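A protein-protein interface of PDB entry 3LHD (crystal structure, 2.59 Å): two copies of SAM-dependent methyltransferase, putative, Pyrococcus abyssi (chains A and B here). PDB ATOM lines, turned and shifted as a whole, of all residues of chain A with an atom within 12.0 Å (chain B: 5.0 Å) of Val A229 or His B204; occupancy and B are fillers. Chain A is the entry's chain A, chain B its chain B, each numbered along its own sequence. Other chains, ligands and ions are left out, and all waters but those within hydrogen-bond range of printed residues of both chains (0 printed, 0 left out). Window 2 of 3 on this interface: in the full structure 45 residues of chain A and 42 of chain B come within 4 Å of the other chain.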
ATOM      1  N   PHE A 225      18.802  26.948  21.396  1.00  0.00           N
ATOM      2  CA  PHE A 225      18.379  27.147  22.768  1.00  0.00           C
ATOM      3  C   PHE A 225      18.128  25.820  23.472  1.00  0.00           C
ATOM      4  O   PHE A 225      17.231  25.076  23.097  1.00  0.00           O
ATOM      5  CB  PHE A 225      17.120  28.012  22.836  1.00  0.00           C
ATOM      6  CG  PHE A 225      17.313  29.408  22.337  1.00  0.00           C
ATOM      7  CD1 PHE A 225      16.521  29.901  21.314  1.00  0.00           C
ATOM      8  CD2 PHE A 225      18.271  30.240  22.893  1.00  0.00           C
ATOM      9  CE1 PHE A 225      16.685  31.202  20.854  1.00  0.00           C
ATOM     10  CE2 PHE A 225      18.442  31.537  22.428  1.00  0.00           C
ATOM     11  CZ  PHE A 225      17.644  32.015  21.411  1.00  0.00           C
ATOM     12  N   ASP A 226      18.939  25.542  24.485  1.00  0.00           N
ATOM     13  CA  ASP A 226      18.690  24.449  25.404  1.00  0.00           C
ATOM     14  C   ASP A 226      17.466  24.731  26.270  1.00  0.00           C
ATOM     15  O   ASP A 226      17.296  25.831  26.786  1.00  0.00           O
ATOM     16  CB  ASP A 226      19.906  24.191  26.289  1.00  0.00           C
ATOM     17  CG  ASP A 226      20.936  23.320  25.617  1.00  0.00           C
ATOM     18  OD1 ASP A 226      21.110  22.159  26.058  1.00  0.00           O
ATOM     19  OD2 ASP A 226      21.565  23.778  24.639  1.00  0.00           O
ATOM     20  N   GLN A 227      16.611  23.723  26.408  1.00  0.00           N
ATOM     21  CA  GLN A 227      15.419  23.830  27.228  1.00  0.00           C
ATOM     22  C   GLN A 227      15.664  23.169  28.563  1.00  0.00           C
ATOM     23  O   GLN A 227      16.320  22.145  28.638  1.00  0.00           O
ATOM     24  CB  GLN A 227      14.228  23.197  26.524  1.00  0.00           C
ATOM     25  CG  GLN A 227      13.853  23.896  25.223  1.00  0.00           C
ATOM     26  CD  GLN A 227      13.488  25.351  25.429  1.00  0.00           C
ATOM     27  OE1 GLN A 227      12.693  25.681  26.305  1.00  0.00           O
ATOM     28  NE2 GLN A 227      14.070  26.228  24.624  1.00  0.00           N
ATOM     29  N   GLU A 228      15.159  23.783  29.620  1.00  0.00           N
ATOM     30  CA  GLU A 228      15.270  23.213  30.947  1.00  0.00           C
ATOM     31  C   GLU A 228      13.914  22.637  31.316  1.00  0.00           C
ATOM     32  O   GLU A 228      12.942  23.367  31.465  1.00  0.00           O
ATOM     33  CB  GLU A 228      15.692  24.278  31.951  1.00  0.00           C
ATOM     34  CG  GLU A 228      16.439  23.723  33.137  1.00  0.00           C
ATOM     35  CD  GLU A 228      16.167  24.502  34.406  1.00  0.00           C
ATOM     36  OE1 GLU A 228      17.126  24.719  35.190  1.00  0.00           O
ATOM     37  OE2 GLU A 228      14.989  24.893  34.619  1.00  0.00           O
ATOM     38  N   VAL A 229      13.844  21.323  31.426  1.00  0.00           N
ATOM     39  CA  VAL A 229      12.577  20.671  31.691  1.00  0.00           C
ATOM     40  C   VAL A 229      12.666  19.950  33.026  1.00  0.00           C
ATOM     41  O   VAL A 229      13.265  18.887  33.125  1.00  0.00           O
ATOM     42  CB  VAL A 229      12.167  19.684  30.553  1.00  0.00           C
ATOM     43  CG1 VAL A 229      10.702  19.314  30.678  1.00  0.00           C
ATOM     44  CG2 VAL A 229      12.426  20.291  29.169  1.00  0.00           C
ATOM     45  N   LYS A 230      12.101  20.559  34.062  1.00  0.00           N
ATOM     46  CA  LYS A 230      11.962  19.898  35.358  1.00  0.00           C
ATOM     47  C   LYS A 230      10.495  19.518  35.512  1.00  0.00           C
ATOM     48  O   LYS A 230       9.647  19.986  34.738  1.00  0.00           O
ATOM     49  CB  LYS A 230      12.436  20.802  36.503  1.00  0.00           C
ATOM     50  CG  LYS A 230      13.706  21.588  36.177  1.00  0.00           C
ATOM     51  CD  LYS A 230      14.736  21.524  37.304  1.00  0.00           C
ATOM     52  CE  LYS A 230      16.142  21.835  36.771  1.00  0.00           C
ATOM     53  NZ  LYS A 230      17.236  21.099  37.491  1.00  0.00           N
ATOM     54  N   LYS A 231      10.190  18.671  36.490  1.00  0.00           N
ATOM     55  CA  LYS A 231       8.820  18.194  36.679  1.00  0.00           C
ATOM     56  C   LYS A 231       7.811  19.344  36.685  1.00  0.00           C
ATOM     57  O   LYS A 231       6.855  19.332  35.908  1.00  0.00           O
ATOM     58  CB  LYS A 231       8.702  17.354  37.957  1.00  0.00           C
ATOM     59  N   GLU A 232       8.056  20.349  37.529  1.00  0.00           N
ATOM     60  CA  GLU A 232       7.091  21.432  37.743  1.00  0.00           C
ATOM     61  C   GLU A 232       7.418  22.754  37.026  1.00  0.00           C
ATOM     62  O   GLU A 232       6.715  23.758  37.220  1.00  0.00           O
ATOM     63  CB  GLU A 232       6.872  21.670  39.251  1.00  0.00           C
ATOM     64  CG  GLU A 232       6.368  20.443  40.050  1.00  0.00           C
ATOM     65  CD  GLU A 232       4.921  20.022  39.724  1.00  0.00           C
ATOM     66  OE1 GLU A 232       4.457  19.005  40.289  1.00  0.00           O
ATOM     67  OE2 GLU A 232       4.248  20.698  38.914  1.00  0.00           O
ATOM     68  N   CYS A 233       8.460  22.762  36.195  1.00  0.00           N
ATOM     69  CA  CYS A 233       8.806  23.977  35.436  1.00  0.00           C
ATOM     70  C   CYS A 233       9.594  23.732  34.145  1.00  0.00           C
ATOM     71  O   CYS A 233      10.681  23.151  34.162  1.00  0.00           O
ATOM     72  CB  CYS A 233       9.538  25.005  36.327  1.00  0.00           C
ATOM     73  SG  CYS A 233      10.091  26.515  35.460  1.00  0.00           S
ATOM     74  N   MET A 234       9.022  24.179  33.030  1.00  0.00           N
ATOM     75  CA  MET A 234       9.736  24.239  31.759  1.00  0.00           C
ATOM     76  C   MET A 234       9.983  25.678  31.320  1.00  0.00           C
ATOM     77  O   MET A 234       9.062  26.498  31.255  1.00  0.00           O
ATOM     78  CB  MET A 234       9.005  23.479  30.655  1.00  0.00           C
ATOM     79  CG  MET A 234       9.904  23.178  29.475  1.00  0.00           C
ATOM     80  SD  MET A 234       9.043  22.777  27.958  1.00  0.00           S
ATOM     81  CE  MET A 234      10.338  23.101  26.758  1.00  0.00           C
ATOM     82  N   ARG A 235      11.243  25.966  31.027  1.00  0.00           N
ATOM     83  CA  ARG A 235      11.679  27.273  30.540  1.00  0.00           C
ATOM     84  C   ARG A 235      12.970  27.088  29.756  1.00  0.00           C
ATOM     85  O   ARG A 235      13.659  26.078  29.930  1.00  0.00           O
ATOM     86  CB  ARG A 235      11.894  28.259  31.701  1.00  0.00           C
ATOM     87  CG  ARG A 235      12.583  27.662  32.916  1.00  0.00           C
ATOM     88  CD  ARG A 235      12.887  28.708  33.965  1.00  0.00           C
ATOM     89  NE  ARG A 235      14.291  29.111  33.924  1.00  0.00           N
ATOM     90  CZ  ARG A 235      15.240  28.613  34.715  1.00  0.00           C
ATOM     91  NH1 ARG A 235      14.941  27.692  35.625  1.00  0.00           N
ATOM     92  NH2 ARG A 235      16.492  29.037  34.596  1.00  0.00           N
ATOM     93  N   PRO A 236      13.302  28.049  28.879  1.00  0.00           N
ATOM     94  CA  PRO A 236      14.617  27.989  28.262  1.00  0.00           C
ATOM     95  C   PRO A 236      15.721  28.161  29.303  1.00  0.00           C
ATOM     96  O   PRO A 236      15.508  28.792  30.335  1.00  0.00           O
ATOM     97  CB  PRO A 236      14.605  29.179  27.299  1.00  0.00           C
ATOM     98  CG  PRO A 236      13.169  29.422  27.009  1.00  0.00           C
ATOM     99  CD  PRO A 236      12.466  29.111  28.290  1.00  0.00           C
ATOM    100  N   ARG A 237      16.881  27.580  29.037  1.00  0.00           N
ATOM    101  CA  ARG A 237      18.060  27.784  29.869  1.00  0.00           C
ATOM    102  C   ARG A 237      18.373  29.287  29.892  1.00  0.00           C
ATOM    103  O   ARG A 237      18.412  29.933  28.841  1.00  0.00           O
ATOM    104  CB  ARG A 237      19.239  26.989  29.300  1.00  0.00           C
ATOM    105  CG  ARG A 237      20.037  26.211  30.328  1.00  0.00           C
ATOM    106  CD  ARG A 237      21.360  25.748  29.729  1.00  0.00           C
ATOM    107  NE  ARG A 237      22.331  26.845  29.648  1.00  0.00           N
ATOM    108  CZ  ARG A 237      23.351  26.906  28.792  1.00  0.00           C
ATOM    109  NH1 ARG A 237      23.554  25.935  27.896  1.00  0.00           N
ATOM    110  NH2 ARG A 237      24.170  27.953  28.826  1.00  0.00           N
ATOM    111  N   THR A 238      18.560  29.826  31.098  1.00  0.00           N
ATOM    112  CA  THR A 238      18.778  31.259  31.344  1.00  0.00           C
ATOM    113  C   THR A 238      19.773  31.885  30.359  1.00  0.00           C
ATOM    114  O   THR A 238      19.492  32.908  29.720  1.00  0.00           O
ATOM    115  CB  THR A 238      19.273  31.470  32.801  1.00  0.00           C
ATOM    116  OG1 THR A 238      18.282  30.982  33.710  1.00  0.00           O
ATOM    117  CG2 THR A 238      19.540  32.940  33.106  1.00  0.00           C
ATOM    118  N   THR A 239      20.926  31.235  30.252  1.00  0.00           N
ATOM    119  CA  THR A 239      22.035  31.647  29.405  1.00  0.00           C
ATOM    120  C   THR A 239      22.125  30.708  28.198  1.00  0.00           C
ATOM    121  O   THR A 239      21.724  29.547  28.281  1.00  0.00           O
ATOM    122  CB  THR A 239      23.341  31.649  30.254  1.00  0.00           C
ATOM    123  OG1 THR A 239      23.519  32.943  30.851  1.00  0.00           O
ATOM    124  CG2 THR A 239      24.576  31.270  29.455  1.00  0.00           C
ATOM    125  N   GLN B 199       3.977  18.621  24.945  1.00  0.00           N
ATOM    126  CA  GLN B 199       4.551  17.372  24.474  1.00  0.00           C
ATOM    127  C   GLN B 199       5.922  17.115  25.089  1.00  0.00           C
ATOM    128  O   GLN B 199       6.216  15.989  25.487  1.00  0.00           O
ATOM    129  CB  GLN B 199       4.647  17.373  22.952  1.00  0.00           C
ATOM    130  CG  GLN B 199       3.315  17.397  22.230  1.00  0.00           C
ATOM    131  CD  GLN B 199       3.476  17.476  20.720  1.00  0.00           C
ATOM    132  OE1 GLN B 199       4.012  18.451  20.185  1.00  0.00           O
ATOM    133  NE2 GLN B 199       3.005  16.452  20.024  1.00  0.00           N
ATOM    134  N   VAL B 200       6.757  18.152  25.169  1.00  0.00           N
ATOM    135  CA  VAL B 200       8.055  18.036  25.833  1.00  0.00           C
ATOM    136  C   VAL B 200       7.874  17.608  27.299  1.00  0.00           C
ATOM    137  O   VAL B 200       8.573  16.714  27.767  1.00  0.00           O
ATOM    138  CB  VAL B 200       8.908  19.336  25.732  1.00  0.00           C
ATOM    139  CG1 VAL B 200      10.274  19.149  26.375  1.00  0.00           C
ATOM    140  CG2 VAL B 200       9.081  19.762  24.289  1.00  0.00           C
ATOM    141  N   MET B 201       6.924  18.225  27.997  1.00  0.00           N
ATOM    142  CA  MET B 201       6.644  17.915  29.408  1.00  0.00           C
ATOM    143  C   MET B 201       6.288  16.440  29.649  1.00  0.00           C
ATOM    144  O   MET B 201       6.769  15.829  30.602  1.00  0.00           O
ATOM    145  CB  MET B 201       5.536  18.830  29.966  1.00  0.00           C
ATOM    146  CG  MET B 201       5.974  20.279  30.249  1.00  0.00           C
ATOM    147  SD  MET B 201       4.622  21.507  30.323  1.00  0.00           S
ATOM    148  CE  MET B 201       3.534  20.775  31.561  1.00  0.00           C
ATOM    149  N   ARG B 202       5.440  15.878  28.794  1.00  0.00           N
ATOM    150  CA  ARG B 202       5.048  14.476  28.905  1.00  0.00           C
ATOM    151  C   ARG B 202       6.201  13.556  28.539  1.00  0.00           C
ATOM    152  O   ARG B 202       6.399  12.513  29.154  1.00  0.00           O
ATOM    153  CB  ARG B 202       3.871  14.181  27.989  1.00  0.00           C
ATOM    154  CG  ARG B 202       2.568  14.822  28.396  1.00  0.00           C
ATOM    155  CD  ARG B 202       1.623  14.769  27.214  1.00  0.00           C
ATOM    156  NE  ARG B 202       0.744  15.935  27.162  1.00  0.00           N
ATOM    157  CZ  ARG B 202       0.381  16.555  26.043  1.00  0.00           C
ATOM    158  NH1 ARG B 202       0.828  16.139  24.859  1.00  0.00           N
ATOM    159  NH2 ARG B 202      -0.422  17.604  26.114  1.00  0.00           N
ATOM    160  N   LEU B 203       6.968  13.955  27.536  1.00  0.00           N
ATOM    161  CA  LEU B 203       8.087  13.156  27.086  1.00  0.00           C
ATOM    162  C   LEU B 203       9.215  13.164  28.109  1.00  0.00           C
ATOM    163  O   LEU B 203       9.951  12.182  28.235  1.00  0.00           O
ATOM    164  CB  LEU B 203       8.574  13.620  25.713  1.00  0.00           C
ATOM    165  CG  LEU B 203       9.832  12.952  25.160  1.00  0.00           C
ATOM    166  CD1 LEU B 203       9.575  11.508  24.798  1.00  0.00           C
ATOM    167  CD2 LEU B 203      10.304  13.726  23.961  1.00  0.00           C
ATOM    168  N   HIS B 204       9.351  14.262  28.844  1.00  0.00           N
ATOM    169  CA  HIS B 204      10.330  14.288  29.916  1.00  0.00           C
ATOM    170  C   HIS B 204       9.855  13.455  31.100  1.00  0.00           C
ATOM    171  O   HIS B 204      10.659  12.800  31.751  1.00  0.00           O
ATOM    172  CB  HIS B 204      10.682  15.706  30.347  1.00  0.00           C
ATOM    173  CG  HIS B 204      11.921  15.777  31.183  1.00  0.00           C
ATOM    174  ND1 HIS B 204      11.888  15.909  32.557  1.00  0.00           N
ATOM    175  CD2 HIS B 204      13.231  15.699  30.842  1.00  0.00           C
ATOM    176  CE1 HIS B 204      13.126  15.920  33.025  1.00  0.00           C
ATOM    177  NE2 HIS B 204      13.959  15.799  32.005  1.00  0.00           N
ATOM    178  N   GLU B 205       8.551  13.477  31.361  1.00  0.00           N
ATOM    179  CA  GLU B 205       7.948  12.632  32.386  1.00  0.00           C
ATOM    180  C   GLU B 205       8.320  11.157  32.136  1.00  0.00           C
ATOM    181  O   GLU B 205       8.878  10.498  33.017  1.00  0.00           O
ATOM    182  CB  GLU B 205       6.419  12.840  32.425  1.00  0.00           C
ATOM    183  CG  GLU B 205       5.719  12.405  33.730  1.00  0.00           C
ATOM    184  CD  GLU B 205       4.182  12.254  33.604  1.00  0.00           C
ATOM    185  OE1 GLU B 205       3.571  12.827  32.664  1.00  0.00           O
ATOM    186  OE2 GLU B 205       3.584  11.551  34.460  1.00  0.00           O
ATOM    187  N   LYS B 206       8.055  10.666  30.923  1.00  0.00           N
ATOM    188  CA  LYS B 206       8.308   9.263  30.561  1.00  0.00           C
ATOM    189  C   LYS B 206       9.784   8.877  30.579  1.00  0.00           C
ATOM    190  O   LYS B 206      10.128   7.766  30.965  1.00  0.00           O
ATOM    191  CB  LYS B 206       7.720   8.944  29.185  1.00  0.00           C
ATOM    192  CG  LYS B 206       7.376   7.476  28.966  1.00  0.00           C
ATOM    193  CD  LYS B 206       6.072   7.125  29.678  1.00  0.00           C
ATOM    194  CE  LYS B 206       5.651   5.700  29.423  1.00  0.00           C
ATOM    195  NZ  LYS B 206       4.381   5.425  30.145  1.00  0.00           N
ATOM    196  N   LEU B 207      10.647   9.790  30.150  1.00  0.00           N
ATOM    197  CA  LEU B 207      12.084   9.534  30.127  1.00  0.00           C
ATOM    198  C   LEU B 207      12.707   9.529  31.528  1.00  0.00           C
ATOM    199  O   LEU B 207      13.740   8.891  31.754  1.00  0.00           O
ATOM    200  CB  LEU B 207      12.799  10.531  29.206  1.00  0.00           C
ATOM    201  CG  LEU B 207      12.609  10.368  27.692  1.00  0.00           C
ATOM    202  CD1 LEU B 207      13.030  11.621  26.949  1.00  0.00           C
ATOM    203  CD2 LEU B 207      13.351   9.155  27.155  1.00  0.00           C
ATOM    204  N   ARG B 208      12.080  10.240  32.464  1.00  0.00           N
ATOM    205  CA  ARG B 208      12.502  10.202  33.861  1.00  0.00           C
ATOM    206  C   ARG B 208      12.173   8.826  34.419  1.00  0.00           C
ATOM    207  O   ARG B 208      13.019   8.174  35.035  1.00  0.00           O
ATOM    208  CB  ARG B 208      11.815  11.302  34.680  1.00  0.00           C
ATOM    209  CG  ARG B 208      12.443  12.682  34.524  1.00  0.00           C
ATOM    210  CD  ARG B 208      11.855  13.709  35.505  1.00  0.00           C
ATOM    211  NE  ARG B 208      10.546  14.227  35.084  1.00  0.00           N
ATOM    212  CZ  ARG B 208       9.422  14.123  35.794  1.00  0.00           C
ATOM    213  NH1 ARG B 208       9.420  13.527  36.989  1.00  0.00           N
ATOM    214  NH2 ARG B 208       8.289  14.627  35.316  1.00  0.00           N
ATOM    215  N   PRO B 217      18.179  13.314  29.324  1.00  0.00           N
ATOM    216  CA  PRO B 217      17.752  13.861  28.045  1.00  0.00           C
ATOM    217  C   PRO B 217      18.114  15.344  27.891  1.00  0.00           C
ATOM    218  O   PRO B 217      18.350  16.027  28.879  1.00  0.00           O
ATOM    219  CB  PRO B 217      16.232  13.642  28.053  1.00  0.00           C
ATOM    220  CG  PRO B 217      15.853  13.518  29.472  1.00  0.00           C
ATOM    221  CD  PRO B 217      17.045  13.018  30.220  1.00  0.00           C
ATOM    222  N   THR B 219      16.819  18.775  25.608  1.00  0.00           N
ATOM    223  CA  THR B 219      15.848  19.339  24.674  1.00  0.00           C
ATOM    224  C   THR B 219      16.356  20.655  24.094  1.00  0.00           C
ATOM    225  O   THR B 219      16.639  21.615  24.827  1.00  0.00           O
ATOM    226  CB  THR B 219      14.464  19.563  25.323  1.00  0.00           C
ATOM    227  OG1 THR B 219      14.011  18.352  25.949  1.00  0.00           O
ATOM    228  CG2 THR B 219      13.451  19.977  24.283  1.00  0.00           C
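Along chain B the printed residues that touch a printed residue of chain A span positions 200 to 219.
Among the printed residues, no Asp or Glu carboxylate lies within 4 Å of a Lys or Arg side-chain nitrogen of the other chain.
Of the printed residues of chain B, Val A229 touches Val B200 and His B204.
His B204 touches just one residue of chain A: Val A229 (3.0 Å).
No residue of chain A comes within 4 Å of Met B201.
No residue of chain A comes within 4 Å of Leu B203.
No residue of chain A comes within 4 Å of Leu B207.
Arg B208 touches just one residue of chain A: Lys A231.
No residue of chain A comes within 4 Å of Pro B217.
Thr B219 touches just these residues of chain A: Phe A225 (3.9 Å), Asp A226 (3.5 Å) and Gln A227 (2.6 Å).
Printed residues of chain B within 4 Å of Phe A225: Thr B219.
Printed residues of chain B within 4 Å of Met A234: Val B200.
Of the printed residues of chain B, Asp A226 touches Thr B219.
Gln B199 touches none of the printed residues of chain A.
Pro A236 touches none of the printed residues of chain B.
The nearest residue of chain B that does not touch Val A229 is Thr B219 (4.1 Å).
The nearest residue of chain A that does not touch His B204 is Lys A230 (4.8 Å).
The nearest printed residue of chain B that does not touch Lys A231 is His B204 (5.1 Å).
N of Gln A227 sits at hydrogen-bond distance from O of Thr B219, 2.6 Å away.
O of Val A229 sits close to ND1 of His B204 (3.3 Å).
Thr B219 touches Phe A225.
C of Asp A226 touches O of Thr B219, 3.5 Å away.
Val B200 touches Val A229 (CG1 to CG2, 3.7 Å).
NH2 of Arg B208 touches CB of Lys A231, 3.8 Å away.
Met A234 touches Val B200.
The guanidinium group (NE) of Arg B208 is in hydrogen-bond range of a ring nitrogen (ND1) of His B204 (3.3 Å).
The backbone NH (N) of Arg A237 sits at hydrogen-bond distance from the backbone carbonyl oxygen (O) of Asp A226, at 2.9 Å.
No position is printed for both chains.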
